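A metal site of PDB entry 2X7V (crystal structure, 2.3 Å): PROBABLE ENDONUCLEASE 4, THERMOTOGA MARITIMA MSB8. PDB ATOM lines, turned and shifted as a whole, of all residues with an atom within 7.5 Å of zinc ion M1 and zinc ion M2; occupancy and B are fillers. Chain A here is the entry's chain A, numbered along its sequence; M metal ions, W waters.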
ATOM      1  N   GLN A  30     -21.704 -36.380   4.990  1.00  0.00           N
ATOM      2  CA  GLN A  30     -22.302 -35.238   4.332  1.00  0.00           C
ATOM      3  C   GLN A  30     -23.100 -35.790   3.150  1.00  0.00           C
ATOM      4  O   GLN A  30     -22.736 -36.804   2.575  1.00  0.00           O
ATOM      5  CB  GLN A  30     -21.201 -34.260   3.898  1.00  0.00           C
ATOM      6  CG  GLN A  30     -21.622 -33.196   2.894  1.00  0.00           C
ATOM      7  CD  GLN A  30     -20.513 -32.215   2.604  1.00  0.00           C
ATOM      8  OE1 GLN A  30     -20.295 -31.257   3.354  1.00  0.00           O
ATOM      9  NE2 GLN A  30     -19.780 -32.451   1.520  1.00  0.00           N
ATOM     10  N   PHE A  32     -25.951 -34.548  -0.283  1.00  0.00           N
ATOM     11  CA  PHE A  32     -26.762 -33.550  -0.962  1.00  0.00           C
ATOM     12  C   PHE A  32     -28.213 -33.692  -0.484  1.00  0.00           C
ATOM     13  O   PHE A  32     -28.677 -34.796  -0.163  1.00  0.00           O
ATOM     14  CB  PHE A  32     -26.693 -33.762  -2.476  1.00  0.00           C
ATOM     15  CG  PHE A  32     -25.370 -33.392  -3.080  1.00  0.00           C
ATOM     16  CD1 PHE A  32     -24.842 -32.132  -2.883  1.00  0.00           C
ATOM     17  CD2 PHE A  32     -24.669 -34.287  -3.862  1.00  0.00           C
ATOM     18  CE1 PHE A  32     -23.619 -31.768  -3.444  1.00  0.00           C
ATOM     19  CE2 PHE A  32     -23.439 -33.950  -4.425  1.00  0.00           C
ATOM     20  CZ  PHE A  32     -22.921 -32.679  -4.204  1.00  0.00           C
ATOM     21  N   HIS A  69     -25.037 -30.607   2.049  1.00  0.00           N
ATOM     22  CA  HIS A  69     -24.257 -29.699   1.236  1.00  0.00           C
ATOM     23  C   HIS A  69     -25.134 -29.227   0.098  1.00  0.00           C
ATOM     24  O   HIS A  69     -25.789 -30.049  -0.530  1.00  0.00           O
ATOM     25  CB  HIS A  69     -23.013 -30.407   0.694  1.00  0.00           C
ATOM     26  CG  HIS A  69     -22.022 -29.495   0.056  1.00  0.00           C
ATOM     27  ND1 HIS A  69     -22.355 -28.619  -0.958  1.00  0.00           N
ATOM     28  CD2 HIS A  69     -20.702 -29.300   0.300  1.00  0.00           C
ATOM     29  CE1 HIS A  69     -21.295 -27.927  -1.314  1.00  0.00           C
ATOM     30  NE2 HIS A  69     -20.278 -28.330  -0.580  1.00  0.00           N
ATOM     31  N   SER A  70     -25.173 -27.931  -0.157  1.00  0.00           N
ATOM     32  CA  SER A  70     -25.947 -27.395  -1.278  1.00  0.00           C
ATOM     33  C   SER A  70     -25.386 -27.805  -2.636  1.00  0.00           C
ATOM     34  O   SER A  70     -24.188 -28.022  -2.786  1.00  0.00           O
ATOM     35  CB  SER A  70     -25.979 -25.875  -1.229  1.00  0.00           C
ATOM     36  OG  SER A  70     -26.667 -25.453  -0.084  1.00  0.00           O
ATOM     37  N   ASN A 107     -24.339 -26.799   4.455  1.00  0.00           N
ATOM     38  CA  ASN A 107     -23.091 -26.207   4.001  1.00  0.00           C
ATOM     39  C   ASN A 107     -23.241 -25.581   2.604  1.00  0.00           C
ATOM     40  O   ASN A 107     -23.811 -26.194   1.709  1.00  0.00           O
ATOM     41  CB  ASN A 107     -22.013 -27.303   3.979  1.00  0.00           C
ATOM     42  CG  ASN A 107     -20.661 -26.793   3.559  1.00  0.00           C
ATOM     43  OD1 ASN A 107     -19.866 -26.329   4.379  1.00  0.00           O
ATOM     44  ND2 ASN A 107     -20.388 -26.850   2.257  1.00  0.00           N
ATOM     45  N   ILE A 108     -22.737 -24.363   2.433  1.00  0.00           N
ATOM     46  CA  ILE A 108     -22.752 -23.699   1.128  1.00  0.00           C
ATOM     47  C   ILE A 108     -21.434 -22.977   0.856  1.00  0.00           C
ATOM     48  O   ILE A 108     -20.727 -22.571   1.780  1.00  0.00           O
ATOM     49  CB  ILE A 108     -23.865 -22.620   0.982  1.00  0.00           C
ATOM     50  CG1 ILE A 108     -23.534 -21.388   1.842  1.00  0.00           C
ATOM     51  CG2 ILE A 108     -25.209 -23.154   1.359  1.00  0.00           C
ATOM     52  CD1 ILE A 108     -24.561 -20.257   1.720  1.00  0.00           C
ATOM     53  N   HIS A 109     -21.135 -22.838  -0.432  1.00  0.00           N
ATOM     54  CA  HIS A 109     -20.126 -21.898  -0.898  1.00  0.00           C
ATOM     55  C   HIS A 109     -20.818 -20.556  -0.968  1.00  0.00           C
ATOM     56  O   HIS A 109     -21.941 -20.461  -1.466  1.00  0.00           O
ATOM     57  CB  HIS A 109     -19.657 -22.309  -2.278  1.00  0.00           C
ATOM     58  CG  HIS A 109     -18.962 -23.639  -2.305  1.00  0.00           C
ATOM     59  ND1 HIS A 109     -18.143 -24.038  -3.335  1.00  0.00           N
ATOM     60  CD2 HIS A 109     -18.943 -24.646  -1.395  1.00  0.00           C
ATOM     61  CE1 HIS A 109     -17.658 -25.238  -3.069  1.00  0.00           C
ATOM     62  NE2 HIS A 109     -18.131 -25.632  -1.894  1.00  0.00           N
ATOM     63  N   GLU A 144     -18.462 -22.091   3.728  1.00  0.00           N
ATOM     64  CA  GLU A 144     -17.251 -22.827   3.459  1.00  0.00           C
ATOM     65  C   GLU A 144     -16.220 -21.966   2.737  1.00  0.00           C
ATOM     66  O   GLU A 144     -16.559 -21.270   1.786  1.00  0.00           O
ATOM     67  CB  GLU A 144     -17.570 -24.041   2.605  1.00  0.00           C
ATOM     68  CG  GLU A 144     -16.340 -24.889   2.346  1.00  0.00           C
ATOM     69  CD  GLU A 144     -16.606 -26.057   1.410  1.00  0.00           C
ATOM     70  OE1 GLU A 144     -17.760 -26.521   1.303  1.00  0.00           O
ATOM     71  OE2 GLU A 144     -15.654 -26.510   0.781  1.00  0.00           O
ATOM     72  N   ASN A 145     -14.971 -21.995   3.161  1.00  0.00           N
ATOM     73  CA  ASN A 145     -13.942 -21.316   2.395  1.00  0.00           C
ATOM     74  C   ASN A 145     -13.779 -21.977   1.018  1.00  0.00           C
ATOM     75  O   ASN A 145     -13.983 -23.183   0.872  1.00  0.00           O
ATOM     76  CB  ASN A 145     -12.602 -21.231   3.142  1.00  0.00           C
ATOM     77  CG  ASN A 145     -11.964 -22.587   3.387  1.00  0.00           C
ATOM     78  OD1 ASN A 145     -10.841 -22.863   2.938  1.00  0.00           O
ATOM     79  ND2 ASN A 145     -12.671 -23.450   4.111  1.00  0.00           N
ATOM     80  N   VAL A 146     -13.461 -21.163   0.010  1.00  0.00           N
ATOM     81  CA  VAL A 146     -13.307 -21.666  -1.351  1.00  0.00           C
ATOM     82  C   VAL A 146     -11.951 -21.266  -1.946  1.00  0.00           C
ATOM     83  O   VAL A 146     -11.171 -20.549  -1.332  1.00  0.00           O
ATOM     84  CB  VAL A 146     -14.451 -21.164  -2.270  1.00  0.00           C
ATOM     85  CG1 VAL A 146     -15.780 -21.764  -1.832  1.00  0.00           C
ATOM     86  CG2 VAL A 146     -14.510 -19.628  -2.265  1.00  0.00           C
ATOM     87  N   THR A 176     -17.399 -23.931   7.797  1.00  0.00           N
ATOM     88  CA  THR A 176     -16.746 -25.176   7.412  1.00  0.00           C
ATOM     89  C   THR A 176     -15.361 -24.814   6.873  1.00  0.00           C
ATOM     90  O   THR A 176     -15.238 -23.879   6.100  1.00  0.00           O
ATOM     91  CB  THR A 176     -17.527 -25.887   6.284  1.00  0.00           C
ATOM     92  OG1 THR A 176     -18.735 -26.451   6.818  1.00  0.00           O
ATOM     93  CG2 THR A 176     -16.682 -27.005   5.634  1.00  0.00           C
ATOM     94  N   TYR A 177     -14.325 -25.543   7.269  1.00  0.00           N
ATOM     95  CA  TYR A 177     -12.998 -25.328   6.712  1.00  0.00           C
ATOM     96  C   TYR A 177     -12.603 -26.481   5.786  1.00  0.00           C
ATOM     97  O   TYR A 177     -12.605 -27.655   6.184  1.00  0.00           O
ATOM     98  CB  TYR A 177     -11.929 -25.175   7.794  1.00  0.00           C
ATOM     99  CG  TYR A 177     -10.577 -24.901   7.196  1.00  0.00           C
ATOM    100  CD1 TYR A 177     -10.271 -23.648   6.687  1.00  0.00           C
ATOM    101  CD2 TYR A 177      -9.608 -25.906   7.110  1.00  0.00           C
ATOM    102  CE1 TYR A 177      -9.046 -23.394   6.108  1.00  0.00           C
ATOM    103  CE2 TYR A 177      -8.374 -25.650   6.560  1.00  0.00           C
ATOM    104  CZ  TYR A 177      -8.096 -24.383   6.049  1.00  0.00           C
ATOM    105  OH  TYR A 177      -6.874 -24.114   5.471  1.00  0.00           O
ATOM    106  N   ASP A 178     -12.272 -26.152   4.543  1.00  0.00           N
ATOM    107  CA  ASP A 178     -11.898 -27.154   3.565  1.00  0.00           C
ATOM    108  C   ASP A 178     -10.395 -27.040   3.408  1.00  0.00           C
ATOM    109  O   ASP A 178      -9.877 -25.978   3.030  1.00  0.00           O
ATOM    110  CB  ASP A 178     -12.623 -26.934   2.232  1.00  0.00           C
ATOM    111  CG  ASP A 178     -12.265 -27.981   1.166  1.00  0.00           C
ATOM    112  OD1 ASP A 178     -13.174 -28.579   0.567  1.00  0.00           O
ATOM    113  OD2 ASP A 178     -11.073 -28.217   0.913  1.00  0.00           O
ATOM    114  N   THR A 179      -9.686 -28.123   3.703  1.00  0.00           N
ATOM    115  CA  THR A 179      -8.228 -28.109   3.722  1.00  0.00           C
ATOM    116  C   THR A 179      -7.626 -27.826   2.353  1.00  0.00           C
ATOM    117  O   THR A 179      -6.620 -27.130   2.256  1.00  0.00           O
ATOM    118  CB  THR A 179      -7.647 -29.414   4.330  1.00  0.00           C
ATOM    119  OG1 THR A 179      -8.083 -30.524   3.561  1.00  0.00           O
ATOM    120  CG2 THR A 179      -8.119 -29.585   5.789  1.00  0.00           C
ATOM    121  N   CYS A 180      -8.240 -28.357   1.301  1.00  0.00           N
ATOM    122  CA  CYS A 180      -7.796 -28.130  -0.079  1.00  0.00           C
ATOM    123  C   CYS A 180      -8.001 -26.672  -0.539  1.00  0.00           C
ATOM    124  O   CYS A 180      -7.069 -26.037  -1.052  1.00  0.00           O
ATOM    125  CB  CYS A 180      -8.458 -29.116  -1.054  1.00  0.00           C
ATOM    126  SG  CYS A 180      -8.013 -28.780  -2.785  1.00  0.00           S
ATOM    127  N   HIS A 181      -9.196 -26.120  -0.331  1.00  0.00           N
ATOM    128  CA  HIS A 181      -9.431 -24.712  -0.664  1.00  0.00           C
ATOM    129  C   HIS A 181      -8.512 -23.775   0.138  1.00  0.00           C
ATOM    130  O   HIS A 181      -7.999 -22.803  -0.403  1.00  0.00           O
ATOM    131  CB  HIS A 181     -10.894 -24.335  -0.436  1.00  0.00           C
ATOM    132  CG  HIS A 181     -11.860 -25.191  -1.195  1.00  0.00           C
ATOM    133  ND1 HIS A 181     -13.173 -25.367  -0.792  1.00  0.00           N
ATOM    134  CD2 HIS A 181     -11.716 -25.904  -2.323  1.00  0.00           C
ATOM    135  CE1 HIS A 181     -13.788 -26.155  -1.644  1.00  0.00           C
ATOM    136  NE2 HIS A 181     -12.927 -26.509  -2.584  1.00  0.00           N
ATOM    137  N   MET A 213     -17.305 -28.143  10.932  1.00  0.00           N
ATOM    138  CA  MET A 213     -16.945 -29.218  10.014  1.00  0.00           C
ATOM    139  C   MET A 213     -15.678 -28.879   9.282  1.00  0.00           C
ATOM    140  O   MET A 213     -15.470 -27.738   8.873  1.00  0.00           O
ATOM    141  CB  MET A 213     -18.076 -29.440   8.987  1.00  0.00           C
ATOM    142  CG  MET A 213     -17.654 -30.296   7.787  1.00  0.00           C
ATOM    143  SD  MET A 213     -19.023 -30.958   6.812  1.00  0.00           S
ATOM    144  CE  MET A 213     -19.888 -29.474   6.266  1.00  0.00           C
ATOM    145  N   ILE A 214     -14.812 -29.872   9.103  1.00  0.00           N
ATOM    146  CA  ILE A 214     -13.676 -29.716   8.221  1.00  0.00           C
ATOM    147  C   ILE A 214     -13.898 -30.597   7.007  1.00  0.00           C
ATOM    148  O   ILE A 214     -14.332 -31.735   7.131  1.00  0.00           O
ATOM    149  CB  ILE A 214     -12.374 -30.094   8.927  1.00  0.00           C
ATOM    150  CG1 ILE A 214     -12.036 -29.029   9.991  1.00  0.00           C
ATOM    151  CG2 ILE A 214     -11.234 -30.181   7.938  1.00  0.00           C
ATOM    152  CD1 ILE A 214     -11.254 -29.536  11.161  1.00  0.00           C
ATOM    153  N   HIS A 215     -13.668 -30.054   5.807  1.00  0.00           N
ATOM    154  CA  HIS A 215     -13.568 -30.924   4.648  1.00  0.00           C
ATOM    155  C   HIS A 215     -12.122 -31.346   4.491  1.00  0.00           C
ATOM    156  O   HIS A 215     -11.247 -30.531   4.240  1.00  0.00           O
ATOM    157  CB  HIS A 215     -14.085 -30.270   3.376  1.00  0.00           C
ATOM    158  CG  HIS A 215     -15.560 -30.105   3.344  1.00  0.00           C
ATOM    159  ND1 HIS A 215     -16.191 -29.185   2.538  1.00  0.00           N
ATOM    160  CD2 HIS A 215     -16.533 -30.737   4.037  1.00  0.00           C
ATOM    161  CE1 HIS A 215     -17.499 -29.271   2.726  1.00  0.00           C
ATOM    162  NE2 HIS A 215     -17.727 -30.203   3.627  1.00  0.00           N
ATOM    163  N   LEU A 216     -11.890 -32.644   4.631  1.00  0.00           N
ATOM    164  CA  LEU A 216     -10.558 -33.190   4.631  1.00  0.00           C
ATOM    165  C   LEU A 216     -10.229 -33.579   3.220  1.00  0.00           C
ATOM    166  O   LEU A 216     -10.648 -34.646   2.749  1.00  0.00           O
ATOM    167  CB  LEU A 216     -10.518 -34.418   5.533  1.00  0.00           C
ATOM    168  CG  LEU A 216      -9.129 -34.785   6.021  1.00  0.00           C
ATOM    169  CD1 LEU A 216      -8.573 -33.616   6.833  1.00  0.00           C
ATOM    170  CD2 LEU A 216      -9.172 -36.104   6.827  1.00  0.00           C
ATOM    171  N   ASN A 217      -9.497 -32.711   2.530  1.00  0.00           N
ATOM    172  CA  ASN A 217      -9.099 -32.959   1.144  1.00  0.00           C
ATOM    173  C   ASN A 217      -7.593 -32.711   0.970  1.00  0.00           C
ATOM    174  O   ASN A 217      -7.076 -31.683   1.401  1.00  0.00           O
ATOM    175  CB  ASN A 217      -9.876 -32.042   0.174  1.00  0.00           C
ATOM    176  CG  ASN A 217     -11.377 -32.212   0.291  1.00  0.00           C
ATOM    177  OD1 ASN A 217     -12.128 -31.232   0.434  1.00  0.00           O
ATOM    178  ND2 ASN A 217     -11.834 -33.459   0.228  1.00  0.00           N
ATOM    179  N   ASP A 228      -8.395 -25.550  -7.068  1.00  0.00           N
ATOM    180  CA  ASP A 228      -9.603 -26.275  -6.695  1.00  0.00           C
ATOM    181  C   ASP A 228      -9.691 -27.687  -7.298  1.00  0.00           C
ATOM    182  O   ASP A 228     -10.683 -28.056  -7.955  1.00  0.00           O
ATOM    183  CB  ASP A 228     -10.841 -25.462  -7.051  1.00  0.00           C
ATOM    184  CG  ASP A 228     -12.096 -26.013  -6.419  1.00  0.00           C
ATOM    185  OD1 ASP A 228     -13.200 -25.765  -6.961  1.00  0.00           O
ATOM    186  OD2 ASP A 228     -11.960 -26.722  -5.391  1.00  0.00           O
ATOM    187  N   HIS A 230      -9.292 -31.482  -5.758  1.00  0.00           N
ATOM    188  CA  HIS A 230      -9.070 -32.334  -4.595  1.00  0.00           C
ATOM    189  C   HIS A 230      -8.257 -33.576  -4.935  1.00  0.00           C
ATOM    190  O   HIS A 230      -8.250 -34.032  -6.073  1.00  0.00           O
ATOM    191  CB  HIS A 230     -10.398 -32.814  -4.026  1.00  0.00           C
ATOM    192  CG  HIS A 230     -11.295 -31.710  -3.569  1.00  0.00           C
ATOM    193  ND1 HIS A 230     -12.532 -31.960  -2.997  1.00  0.00           N
ATOM    194  CD2 HIS A 230     -11.157 -30.368  -3.598  1.00  0.00           C
ATOM    195  CE1 HIS A 230     -13.109 -30.808  -2.696  1.00  0.00           C
ATOM    196  NE2 HIS A 230     -12.294 -29.830  -3.039  1.00  0.00           N
ATOM    197  N   ILE A 258     -14.654 -34.525   7.176  1.00  0.00           N
ATOM    198  CA  ILE A 258     -15.457 -35.053   6.089  1.00  0.00           C
ATOM    199  C   ILE A 258     -14.618 -35.114   4.796  1.00  0.00           C
ATOM    200  O   ILE A 258     -14.200 -34.087   4.272  1.00  0.00           O
ATOM    201  CB  ILE A 258     -16.748 -34.180   5.883  1.00  0.00           C
ATOM    202  CG1 ILE A 258     -17.587 -34.156   7.167  1.00  0.00           C
ATOM    203  CG2 ILE A 258     -17.578 -34.660   4.687  1.00  0.00           C
ATOM    204  CD1 ILE A 258     -18.175 -35.485   7.527  1.00  0.00           C
ATOM    205  N   GLU A 260     -13.937 -35.352   0.936  1.00  0.00           N
ATOM    206  CA  GLU A 260     -14.557 -35.076  -0.360  1.00  0.00           C
ATOM    207  C   GLU A 260     -13.564 -35.388  -1.470  1.00  0.00           C
ATOM    208  O   GLU A 260     -13.538 -34.746  -2.504  1.00  0.00           O
ATOM    209  CB  GLU A 260     -14.959 -33.611  -0.475  1.00  0.00           C
ATOM    210  CG  GLU A 260     -15.951 -33.119   0.554  1.00  0.00           C
ATOM    211  CD  GLU A 260     -16.268 -31.671   0.308  1.00  0.00           C
ATOM    212  OE1 GLU A 260     -15.296 -30.883   0.280  1.00  0.00           O
ATOM    213  OE2 GLU A 260     -17.460 -31.313   0.104  1.00  0.00           O
HETATM  214 ZN    ZN M   1     -15.262 -28.711   0.406  1.00  0.00          ZN
HETATM  215 ZN    ZN M   2     -18.191 -27.455  -0.682  1.00  0.00          ZN
HETATM  216 ZN    ZN M   3     -13.308 -28.098  -3.990  1.00  0.00          ZN
HETATM  217  O   HOH W   1     -16.692 -29.046  -1.247  1.00  0.00           O
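ND2 of Asn 107 touches zinc ion M2, 3.7 Å away. Within 4 Å of zinc ion M2: His 69, Asn 107, His 109, Glu 144 and His 215. The nearest printed residue that does not touch zinc ion M2 is Glu 260 (4.005 Å).
His 181 touches zinc ion M1 (CE1 to ZN, 3.6 Å). Five residues have an atom within 4 Å of zinc ion M1: Glu 144, Asp 178, His 181, His 215 and Glu 260. The nearest printed residue that does not touch zinc ion M1 is Asn 217 (4.02 Å).
The side-chain carboxylate of Asp 178 is in hydrogen-bond range of the backbone NH of His 181 (3.1 Å). The side-chain carboxylate of Asp 178 lies close to the side-chain amide oxygen of Asn 217 (3.2 Å). The backbone NH (N) of Glu 260 lies close to the side-chain amide nitrogen (ND2) of Asn 217 (2.9 Å). The backbone carbonyl oxygen of Glu 260 lies within hydrogen-bond range of a ring nitrogen (ND1) of His 230 (3.0 Å). O of Ile 108 is in hydrogen-bond range of N of Glu 144 (3.0 Å). ND2 of Asn 107 lies close to NE2 of His 69, 3.2 Å away. ND1 of His 181 lies within hydrogen-bond range of O of Asn 145, at 2.9 Å. The side-chain amide oxygen (OD1) of Asn 107 sits at hydrogen-bond distance from the side-chain hydroxyl (OG1) of Thr 176 (2.7 Å).
Zinc ion M1 is bound by the side-chain carboxylate (OD1) of Asp 178 (2.1 Å), the side-chain carboxylate (OE1) of Glu 260 (2.2 Å), water W1 (2.2 Å), the side-chain carboxylate (OE2) of Glu 144 (2.3 Å) and a ring nitrogen (ND1) of His 215 (2.4 Å). Zinc ion M1 has five donor atoms within binding distance.
Zinc ion M2 is bound by a ring nitrogen (NE2) of His 109 (2.2 Å), the side-chain carboxylate of Glu 144 (2.2 Å), water W1 (2.3 Å) and a ring nitrogen (NE2) of His 69 (2.3 Å). Zinc ion M2 has four donor atoms within binding distance.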
